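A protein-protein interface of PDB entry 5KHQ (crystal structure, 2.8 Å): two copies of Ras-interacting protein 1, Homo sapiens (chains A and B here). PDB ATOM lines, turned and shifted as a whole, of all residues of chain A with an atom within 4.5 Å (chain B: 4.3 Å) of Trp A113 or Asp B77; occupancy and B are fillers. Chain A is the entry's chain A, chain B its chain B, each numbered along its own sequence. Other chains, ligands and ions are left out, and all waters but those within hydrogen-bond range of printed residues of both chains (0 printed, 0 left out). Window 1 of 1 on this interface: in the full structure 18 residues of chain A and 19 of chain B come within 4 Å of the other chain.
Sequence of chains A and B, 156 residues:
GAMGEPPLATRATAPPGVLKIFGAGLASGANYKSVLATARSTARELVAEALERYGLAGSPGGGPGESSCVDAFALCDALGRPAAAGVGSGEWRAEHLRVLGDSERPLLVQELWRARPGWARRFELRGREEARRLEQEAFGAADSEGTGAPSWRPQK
The backbone carbonyl oxygen (O) of Glu A111 lies close to the guanidinium group (NE) of Arg B116. The backbone carbonyl oxygen (O) of Leu A112 lies within hydrogen-bond range of the backbone NH (N) of Arg B116 (3.1 Å). The indole nitrogen of Trp A113 sits at hydrogen-bond distance from the side-chain carboxylate of Asp B77. The backbone carbonyl oxygen (O) of Arg B114 is in hydrogen-bond range of the backbone NH (N) of Arg A114.
The backbone carbonyl oxygen of Val A109 lies within hydrogen-bond range of the guanidinium group of Arg A121 (2.7 Å). The side-chain amide nitrogen of Gln A110 is in hydrogen-bond range of the side-chain carboxylate of Glu A111, 3.0 Å away. The backbone carbonyl oxygen (O) of Trp A113 sits at hydrogen-bond distance from the guanidinium group (NH1) of Arg A121, 2.7 Å away. The backbone NH (N) of Arg B98 is in hydrogen-bond range of the backbone carbonyl oxygen (O) of Asp B77, at 2.8 Å. The side-chain carboxylate of Asp B77 is in salt-bridge range of the guanidinium group of Arg B121, at 2.8 Å. O of Trp B113 sits at hydrogen-bond distance from NH2 of Arg B121 (2.6 Å).
Leu A108 touches His B96. O of Leu A112 touches CD1 of Leu B79 (3.6 Å). CD1 of Leu A112 touches ND1 of His B96, at 3.4 Å. Trp A113 touches Leu B79. Arg B114 touches Trp A113 (O to CA, 3.4 Å). Trp A113 touches Arg B121 (NE1 to NE, 3.6 Å). O of Arg A114 touches CA of Trp B113, at 3.3 Å. Arg B116 touches Arg A114 (CA to NE, 3.7 Å). Arg A121 touches Trp B113 (NE to NE1, 3.9 Å).
Trp A113 touches just these residues of chain B: Asp B77, Leu B79, Arg B114 and Arg B121. Of the printed residues of chain B, Arg A114 touches Trp B113, Arg B114 and Arg B116. Of the printed residues of chain B, Arg A121 touches Trp B113 (3.9 Å). Printed residues of chain A within 4 Å of Asp B77: Trp A113. Of the printed residues of chain A, Leu B79 touches Leu A112 and Trp A113. Leu B97 touches none of the printed residues of chain A. Arg B98 touches none of the printed residues of chain A. Of the printed residues of chain A, Trp B113 touches Arg A114 and Arg A121. Printed residues of chain A within 4 Å of Arg B116: Glu A111, Leu A112 and Arg A114. The nearest printed residue of chain B that does not touch Trp A113 is His B96 (4.1 Å). The nearest printed residue of chain B that does not touch Arg A114 is Arg B121 (6.7 Å).
Of the 8 printed residues of chain A, 6 touch a printed residue of chain B. Printed residues of chain B that touch a printed residue of chain A: Asp B77, Leu B79, His B96, Trp B113, Arg B114, Arg B116 and Arg B121. Hydrophobic or aromatic side chains of chain B that line the printed part of chain A: Leu B79, His B96 and Trp B113. Among the printed residues, 13 pairs touch across the chains. Among the printed residues, no Asp or Glu carboxylate lies within 4 Å of a Lys or Arg side-chain nitrogen of the other chain.
Trp A113 touches Arg B114, and with the chains exchanged Arg A114 touches Trp B113. Trp A113 touches Arg B121, and with the chains exchanged Arg A121 touches Trp B113. Arg B114 touches its own counterpart, Arg A114. Positions printed for both chains: 109, 113, 114 and 121.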
ATOM      1  N   LEU A 108       2.151  -2.956   3.623  1.00  0.00           N
ATOM      2  CA  LEU A 108       2.573  -3.769   2.476  1.00  0.00           C
ATOM      3  C   LEU A 108       2.098  -5.216   2.580  1.00  0.00           C
ATOM      4  O   LEU A 108       1.689  -5.806   1.575  1.00  0.00           O
ATOM      5  CB  LEU A 108       4.090  -3.725   2.284  1.00  0.00           C
ATOM      6  CG  LEU A 108       4.842  -2.404   2.051  1.00  0.00           C
ATOM      7  CD1 LEU A 108       6.247  -2.744   1.579  1.00  0.00           C
ATOM      8  CD2 LEU A 108       4.150  -1.455   1.075  1.00  0.00           C
ATOM      9  N   VAL A 109       2.142  -5.773   3.792  1.00  0.00           N
ATOM     10  CA  VAL A 109       1.615  -7.113   4.076  1.00  0.00           C
ATOM     11  C   VAL A 109       0.152  -7.202   3.663  1.00  0.00           C
ATOM     12  O   VAL A 109      -0.245  -8.152   2.998  1.00  0.00           O
ATOM     13  CB  VAL A 109       1.761  -7.489   5.562  1.00  0.00           C
ATOM     14  CG1 VAL A 109       1.145  -8.846   5.830  1.00  0.00           C
ATOM     15  CG2 VAL A 109       3.224  -7.479   5.990  1.00  0.00           C
ATOM     16  N   GLN A 110      -0.632  -6.190   4.024  1.00  0.00           N
ATOM     17  CA  GLN A 110      -2.057  -6.172   3.709  1.00  0.00           C
ATOM     18  C   GLN A 110      -2.352  -5.933   2.234  1.00  0.00           C
ATOM     19  O   GLN A 110      -3.280  -6.520   1.699  1.00  0.00           O
ATOM     20  CB  GLN A 110      -2.793  -5.138   4.552  1.00  0.00           C
ATOM     21  CG  GLN A 110      -4.301  -5.200   4.387  1.00  0.00           C
ATOM     22  CD  GLN A 110      -4.974  -3.995   4.963  1.00  0.00           C
ATOM     23  OE1 GLN A 110      -5.335  -3.974   6.141  1.00  0.00           O
ATOM     24  NE2 GLN A 110      -5.146  -2.972   4.138  1.00  0.00           N
ATOM     25  N   GLU A 111      -1.562  -5.089   1.583  1.00  0.00           N
ATOM     26  CA  GLU A 111      -1.883  -4.670   0.221  1.00  0.00           C
ATOM     27  C   GLU A 111      -1.271  -5.508  -0.901  1.00  0.00           C
ATOM     28  O   GLU A 111      -1.890  -5.645  -1.954  1.00  0.00           O
ATOM     29  CB  GLU A 111      -1.614  -3.175   0.022  1.00  0.00           C
ATOM     30  CG  GLU A 111      -2.550  -2.252   0.812  1.00  0.00           C
ATOM     31  CD  GLU A 111      -4.034  -2.356   0.434  1.00  0.00           C
ATOM     32  OE1 GLU A 111      -4.372  -2.681  -0.730  1.00  0.00           O
ATOM     33  OE2 GLU A 111      -4.881  -2.095   1.313  1.00  0.00           O
ATOM     34  N   LEU A 112      -0.086  -6.076  -0.671  1.00  0.00           N
ATOM     35  CA  LEU A 112       0.617  -6.887  -1.684  1.00  0.00           C
ATOM     36  C   LEU A 112       0.249  -8.371  -1.677  1.00  0.00           C
ATOM     37  O   LEU A 112       0.565  -9.092  -2.627  1.00  0.00           O
ATOM     38  CB  LEU A 112       2.137  -6.724  -1.567  1.00  0.00           C
ATOM     39  CG  LEU A 112       2.743  -5.326  -1.734  1.00  0.00           C
ATOM     40  CD1 LEU A 112       4.216  -5.374  -1.372  1.00  0.00           C
ATOM     41  CD2 LEU A 112       2.554  -4.755  -3.135  1.00  0.00           C
ATOM     42  N   TRP A 113      -0.410  -8.814  -0.605  1.00  0.00           N
ATOM     43  CA  TRP A 113      -0.943 -10.169  -0.512  1.00  0.00           C
ATOM     44  C   TRP A 113      -2.452 -10.180  -0.270  1.00  0.00           C
ATOM     45  O   TRP A 113      -3.019  -9.214   0.238  1.00  0.00           O
ATOM     46  CB  TRP A 113      -0.252 -10.929   0.606  1.00  0.00           C
ATOM     47  CG  TRP A 113       1.105 -11.450   0.269  1.00  0.00           C
ATOM     48  CD1 TRP A 113       1.399 -12.608  -0.397  1.00  0.00           C
ATOM     49  CD2 TRP A 113       2.359 -10.857   0.614  1.00  0.00           C
ATOM     50  NE1 TRP A 113       2.761 -12.772  -0.493  1.00  0.00           N
ATOM     51  CE2 TRP A 113       3.375 -11.711   0.117  1.00  0.00           C
ATOM     52  CE3 TRP A 113       2.728  -9.687   1.295  1.00  0.00           C
ATOM     53  CZ2 TRP A 113       4.737 -11.430   0.277  1.00  0.00           C
ATOM     54  CZ3 TRP A 113       4.083  -9.408   1.457  1.00  0.00           C
ATOM     55  CH2 TRP A 113       5.071 -10.278   0.948  1.00  0.00           C
ATOM     56  N   ARG A 114      -3.080 -11.292  -0.649  1.00  0.00           N
ATOM     57  CA  ARG A 114      -4.499 -11.565  -0.429  1.00  0.00           C
ATOM     58  C   ARG A 114      -4.645 -12.872   0.337  1.00  0.00           C
ATOM     59  O   ARG A 114      -3.695 -13.666   0.410  1.00  0.00           O
ATOM     60  CB  ARG A 114      -5.205 -11.736  -1.769  1.00  0.00           C
ATOM     61  CG  ARG A 114      -5.597 -10.452  -2.470  1.00  0.00           C
ATOM     62  CD  ARG A 114      -6.481 -10.775  -3.666  1.00  0.00           C
ATOM     63  NE  ARG A 114      -5.713 -10.980  -4.895  1.00  0.00           N
ATOM     64  CZ  ARG A 114      -5.981 -11.889  -5.833  1.00  0.00           C
ATOM     65  NH1 ARG A 114      -6.994 -12.739  -5.697  1.00  0.00           N
ATOM     66  NH2 ARG A 114      -5.208 -11.963  -6.911  1.00  0.00           N
ATOM     67  N   ARG A 121      -9.587 -12.549   6.151  1.00  0.00           N
ATOM     68  CA  ARG A 121      -8.308 -12.048   6.634  1.00  0.00           C
ATOM     69  C   ARG A 121      -8.444 -10.792   7.490  1.00  0.00           C
ATOM     70  O   ARG A 121      -9.189  -9.869   7.132  1.00  0.00           O
ATOM     71  CB  ARG A 121      -7.439 -11.736   5.428  1.00  0.00           C
ATOM     72  CG  ARG A 121      -5.995 -11.467   5.754  1.00  0.00           C
ATOM     73  CD  ARG A 121      -5.317 -10.928   4.524  1.00  0.00           C
ATOM     74  NE  ARG A 121      -3.886 -10.798   4.729  1.00  0.00           N
ATOM     75  CZ  ARG A 121      -3.087 -10.099   3.935  1.00  0.00           C
ATOM     76  NH1 ARG A 121      -3.584  -9.462   2.871  1.00  0.00           N
ATOM     77  NH2 ARG A 121      -1.796 -10.033   4.218  1.00  0.00           N
ATOM     78  N   CYS B  76      12.478 -17.133   0.780  1.00  0.00           N
ATOM     79  CA  CYS B  76      11.777 -15.861   0.636  1.00  0.00           C
ATOM     80  C   CYS B  76      10.522 -15.991  -0.192  1.00  0.00           C
ATOM     81  O   CYS B  76      10.548 -16.563  -1.274  1.00  0.00           O
ATOM     82  CB  CYS B  76      12.683 -14.808  -0.004  1.00  0.00           C
ATOM     83  SG  CYS B  76      14.276 -14.590   0.818  1.00  0.00           S
ATOM     84  N   ASP B  77       9.426 -15.456   0.335  1.00  0.00           N
ATOM     85  CA  ASP B  77       8.220 -15.232  -0.435  1.00  0.00           C
ATOM     86  C   ASP B  77       8.496 -13.925  -1.179  1.00  0.00           C
ATOM     87  O   ASP B  77       8.596 -12.867  -0.549  1.00  0.00           O
ATOM     88  CB  ASP B  77       7.008 -15.136   0.510  1.00  0.00           C
ATOM     89  CG  ASP B  77       5.651 -15.185  -0.221  1.00  0.00           C
ATOM     90  OD1 ASP B  77       5.593 -15.199  -1.476  1.00  0.00           O
ATOM     91  OD2 ASP B  77       4.615 -15.205   0.485  1.00  0.00           O
ATOM     92  N   ALA B  78       8.673 -14.009  -2.504  1.00  0.00           N
ATOM     93  CA  ALA B  78       9.021 -12.847  -3.347  1.00  0.00           C
ATOM     94  C   ALA B  78       7.919 -12.466  -4.336  1.00  0.00           C
ATOM     95  O   ALA B  78       7.251 -13.341  -4.884  1.00  0.00           O
ATOM     96  CB  ALA B  78      10.318 -13.114  -4.084  1.00  0.00           C
ATOM     97  N   LEU B  79       7.747 -11.163  -4.564  1.00  0.00           N
ATOM     98  CA  LEU B  79       6.706 -10.636  -5.464  1.00  0.00           C
ATOM     99  C   LEU B  79       7.249  -9.640  -6.493  1.00  0.00           C
ATOM    100  O   LEU B  79       8.147  -8.861  -6.183  1.00  0.00           O
ATOM    101  CB  LEU B  79       5.595  -9.950  -4.664  1.00  0.00           C
ATOM    102  CG  LEU B  79       4.935 -10.580  -3.436  1.00  0.00           C
ATOM    103  CD1 LEU B  79       4.136  -9.512  -2.715  1.00  0.00           C
ATOM    104  CD2 LEU B  79       4.040 -11.755  -3.789  1.00  0.00           C
ATOM    105  N   HIS B  96       9.329  -6.710  -4.126  1.00  0.00           N
ATOM    106  CA  HIS B  96       9.321  -6.818  -2.669  1.00  0.00           C
ATOM    107  C   HIS B  96       9.490  -8.287  -2.268  1.00  0.00           C
ATOM    108  O   HIS B  96       9.210  -9.185  -3.069  1.00  0.00           O
ATOM    109  CB  HIS B  96       8.032  -6.207  -2.076  1.00  0.00           C
ATOM    110  CG  HIS B  96       7.998  -6.194  -0.572  1.00  0.00           C
ATOM    111  ND1 HIS B  96       6.960  -6.740   0.154  1.00  0.00           N
ATOM    112  CD2 HIS B  96       8.888  -5.727   0.340  1.00  0.00           C
ATOM    113  CE1 HIS B  96       7.203  -6.595   1.445  1.00  0.00           C
ATOM    114  NE2 HIS B  96       8.367  -5.988   1.585  1.00  0.00           N
ATOM    115  N   LEU B  97       9.972  -8.530  -1.050  1.00  0.00           N
ATOM    116  CA  LEU B  97      10.041  -9.881  -0.525  1.00  0.00           C
ATOM    117  C   LEU B  97       9.887  -9.983   0.994  1.00  0.00           C
ATOM    118  O   LEU B  97      10.034  -8.995   1.707  1.00  0.00           O
ATOM    119  CB  LEU B  97      11.313 -10.596  -1.010  1.00  0.00           C
ATOM    120  CG  LEU B  97      12.751 -10.241  -0.631  1.00  0.00           C
ATOM    121  CD1 LEU B  97      13.128 -10.619   0.799  1.00  0.00           C
ATOM    122  CD2 LEU B  97      13.649 -10.983  -1.608  1.00  0.00           C
ATOM    123  N   ARG B  98       9.598 -11.195   1.470  1.00  0.00           N
ATOM    124  CA  ARG B  98       9.540 -11.494   2.888  1.00  0.00           C
ATOM    125  C   ARG B  98      10.383 -12.731   3.200  1.00  0.00           C
ATOM    126  O   ARG B  98      10.192 -13.793   2.595  1.00  0.00           O
ATOM    127  CB  ARG B  98       8.088 -11.714   3.331  1.00  0.00           C
ATOM    128  CG  ARG B  98       7.951 -12.079   4.800  1.00  0.00           C
ATOM    129  CD  ARG B  98       6.504 -12.279   5.177  1.00  0.00           C
ATOM    130  NE  ARG B  98       5.977 -13.632   4.949  1.00  0.00           N
ATOM    131  CZ  ARG B  98       6.267 -14.717   5.678  1.00  0.00           C
ATOM    132  NH1 ARG B  98       7.133 -14.664   6.676  1.00  0.00           N
ATOM    133  NH2 ARG B  98       5.695 -15.871   5.397  1.00  0.00           N
ATOM    134  N   LEU B 100      11.017 -15.815   5.183  1.00  0.00           N
ATOM    135  CA  LEU B 100      10.306 -16.789   6.011  1.00  0.00           C
ATOM    136  C   LEU B 100      11.061 -17.181   7.275  1.00  0.00           C
ATOM    137  O   LEU B 100      12.289 -17.319   7.268  1.00  0.00           O
ATOM    138  CB  LEU B 100       9.970 -18.033   5.201  1.00  0.00           C
ATOM    139  CG  LEU B 100       8.577 -18.009   4.585  1.00  0.00           C
ATOM    140  CD1 LEU B 100       8.530 -17.178   3.310  1.00  0.00           C
ATOM    141  CD2 LEU B 100       8.118 -19.436   4.324  1.00  0.00           C
ATOM    142  N   VAL B 109       2.128 -21.086   3.463  1.00  0.00           N
ATOM    143  CA  VAL B 109       2.416 -19.734   2.953  1.00  0.00           C
ATOM    144  C   VAL B 109       2.044 -19.647   1.468  1.00  0.00           C
ATOM    145  O   VAL B 109       1.362 -18.706   1.041  1.00  0.00           O
ATOM    146  CB  VAL B 109       3.895 -19.339   3.148  1.00  0.00           C
ATOM    147  CG1 VAL B 109       4.160 -17.940   2.602  1.00  0.00           C
ATOM    148  CG2 VAL B 109       4.301 -19.427   4.614  1.00  0.00           C
ATOM    149  N   TRP B 113      -2.180 -17.835   1.273  1.00  0.00           N
ATOM    150  CA  TRP B 113      -2.082 -16.492   0.702  1.00  0.00           C
ATOM    151  C   TRP B 113      -1.834 -16.540  -0.790  1.00  0.00           C
ATOM    152  O   TRP B 113      -1.178 -17.449  -1.285  1.00  0.00           O
ATOM    153  CB  TRP B 113      -0.968 -15.692   1.360  1.00  0.00           C
ATOM    154  CG  TRP B 113      -1.254 -15.315   2.768  1.00  0.00           C
ATOM    155  CD1 TRP B 113      -1.989 -14.244   3.200  1.00  0.00           C
ATOM    156  CD2 TRP B 113      -0.798 -15.993   3.943  1.00  0.00           C
ATOM    157  NE1 TRP B 113      -2.018 -14.215   4.573  1.00  0.00           N
ATOM    158  CE2 TRP B 113      -1.298 -15.277   5.057  1.00  0.00           C
ATOM    159  CE3 TRP B 113      -0.014 -17.137   4.166  1.00  0.00           C
ATOM    160  CZ2 TRP B 113      -1.033 -15.665   6.384  1.00  0.00           C
ATOM    161  CZ3 TRP B 113       0.246 -17.534   5.491  1.00  0.00           C
ATOM    162  CH2 TRP B 113      -0.267 -16.798   6.580  1.00  0.00           C
ATOM    163  N   ARG B 114      -2.376 -15.549  -1.488  1.00  0.00           N
ATOM    164  CA  ARG B 114      -2.119 -15.321  -2.903  1.00  0.00           C
ATOM    165  C   ARG B 114      -1.483 -13.934  -3.048  1.00  0.00           C
ATOM    166  O   ARG B 114      -1.601 -13.093  -2.149  1.00  0.00           O
ATOM    167  CB  ARG B 114      -3.432 -15.402  -3.692  1.00  0.00           C
ATOM    168  N   ARG B 116      -1.411 -10.193  -4.674  1.00  0.00           N
ATOM    169  CA  ARG B 116      -2.453  -9.252  -5.112  1.00  0.00           C
ATOM    170  C   ARG B 116      -2.603  -9.335  -6.643  1.00  0.00           C
ATOM    171  O   ARG B 116      -1.664  -9.784  -7.310  1.00  0.00           O
ATOM    172  CB  ARG B 116      -2.151  -7.819  -4.621  1.00  0.00           C
ATOM    173  CG  ARG B 116      -1.424  -6.918  -5.613  1.00  0.00           C
ATOM    174  CD  ARG B 116      -1.432  -5.441  -5.229  1.00  0.00           C
ATOM    175  NE  ARG B 116      -2.780  -4.867  -5.116  1.00  0.00           N
ATOM    176  CZ  ARG B 116      -3.053  -3.574  -4.918  1.00  0.00           C
ATOM    177  NH1 ARG B 116      -2.082  -2.674  -4.817  1.00  0.00           N
ATOM    178  NH2 ARG B 116      -4.315  -3.173  -4.826  1.00  0.00           N
ATOM    179  N   ARG B 121       4.594 -14.135  -8.126  1.00  0.00           N
ATOM    180  CA  ARG B 121       4.962 -14.579  -6.793  1.00  0.00           C
ATOM    181  C   ARG B 121       5.767 -15.854  -6.935  1.00  0.00           C
ATOM    182  O   ARG B 121       5.415 -16.703  -7.751  1.00  0.00           O
ATOM    183  CB  ARG B 121       3.694 -14.811  -5.958  1.00  0.00           C
ATOM    184  CG  ARG B 121       3.890 -15.573  -4.659  1.00  0.00           C
ATOM    185  CD  ARG B 121       2.695 -15.383  -3.756  1.00  0.00           C
ATOM    186  NE  ARG B 121       3.013 -15.810  -2.401  1.00  0.00           N
ATOM    187  CZ  ARG B 121       2.319 -16.708  -1.712  1.00  0.00           C
ATOM    188  NH1 ARG B 121       2.703 -17.030  -0.480  1.00  0.00           N
ATOM    189  NH2 ARG B 121       1.242 -17.280  -2.244  1.00  0.00           N
ATOM    190  N   ARG B 122       6.839 -15.984  -6.151  1.00  0.00           N
ATOM    191  CA  ARG B 122       7.679 -17.185  -6.158  1.00  0.00           C
ATOM    192  C   ARG B 122       8.588 -17.274  -4.937  1.00  0.00           C
ATOM    193  O   ARG B 122       8.974 -16.250  -4.370  1.00  0.00           O
ATOM    194  CB  ARG B 122       8.521 -17.275  -7.442  1.00  0.00           C
ATOM    195  CG  ARG B 122       9.326 -16.028  -7.754  1.00  0.00           C
ATOM    196  CD  ARG B 122      10.733 -16.357  -8.213  1.00  0.00           C
ATOM    197  NE  ARG B 122      10.927 -16.123  -9.644  1.00  0.00           N
ATOM    198  CZ  ARG B 122      12.112 -15.948 -10.228  1.00  0.00           C
ATOM    199  NH1 ARG B 122      12.173 -15.741 -11.537  1.00  0.00           N
ATOM    200  NH2 ARG B 122      13.236 -15.963  -9.512  1.00  0.00           N
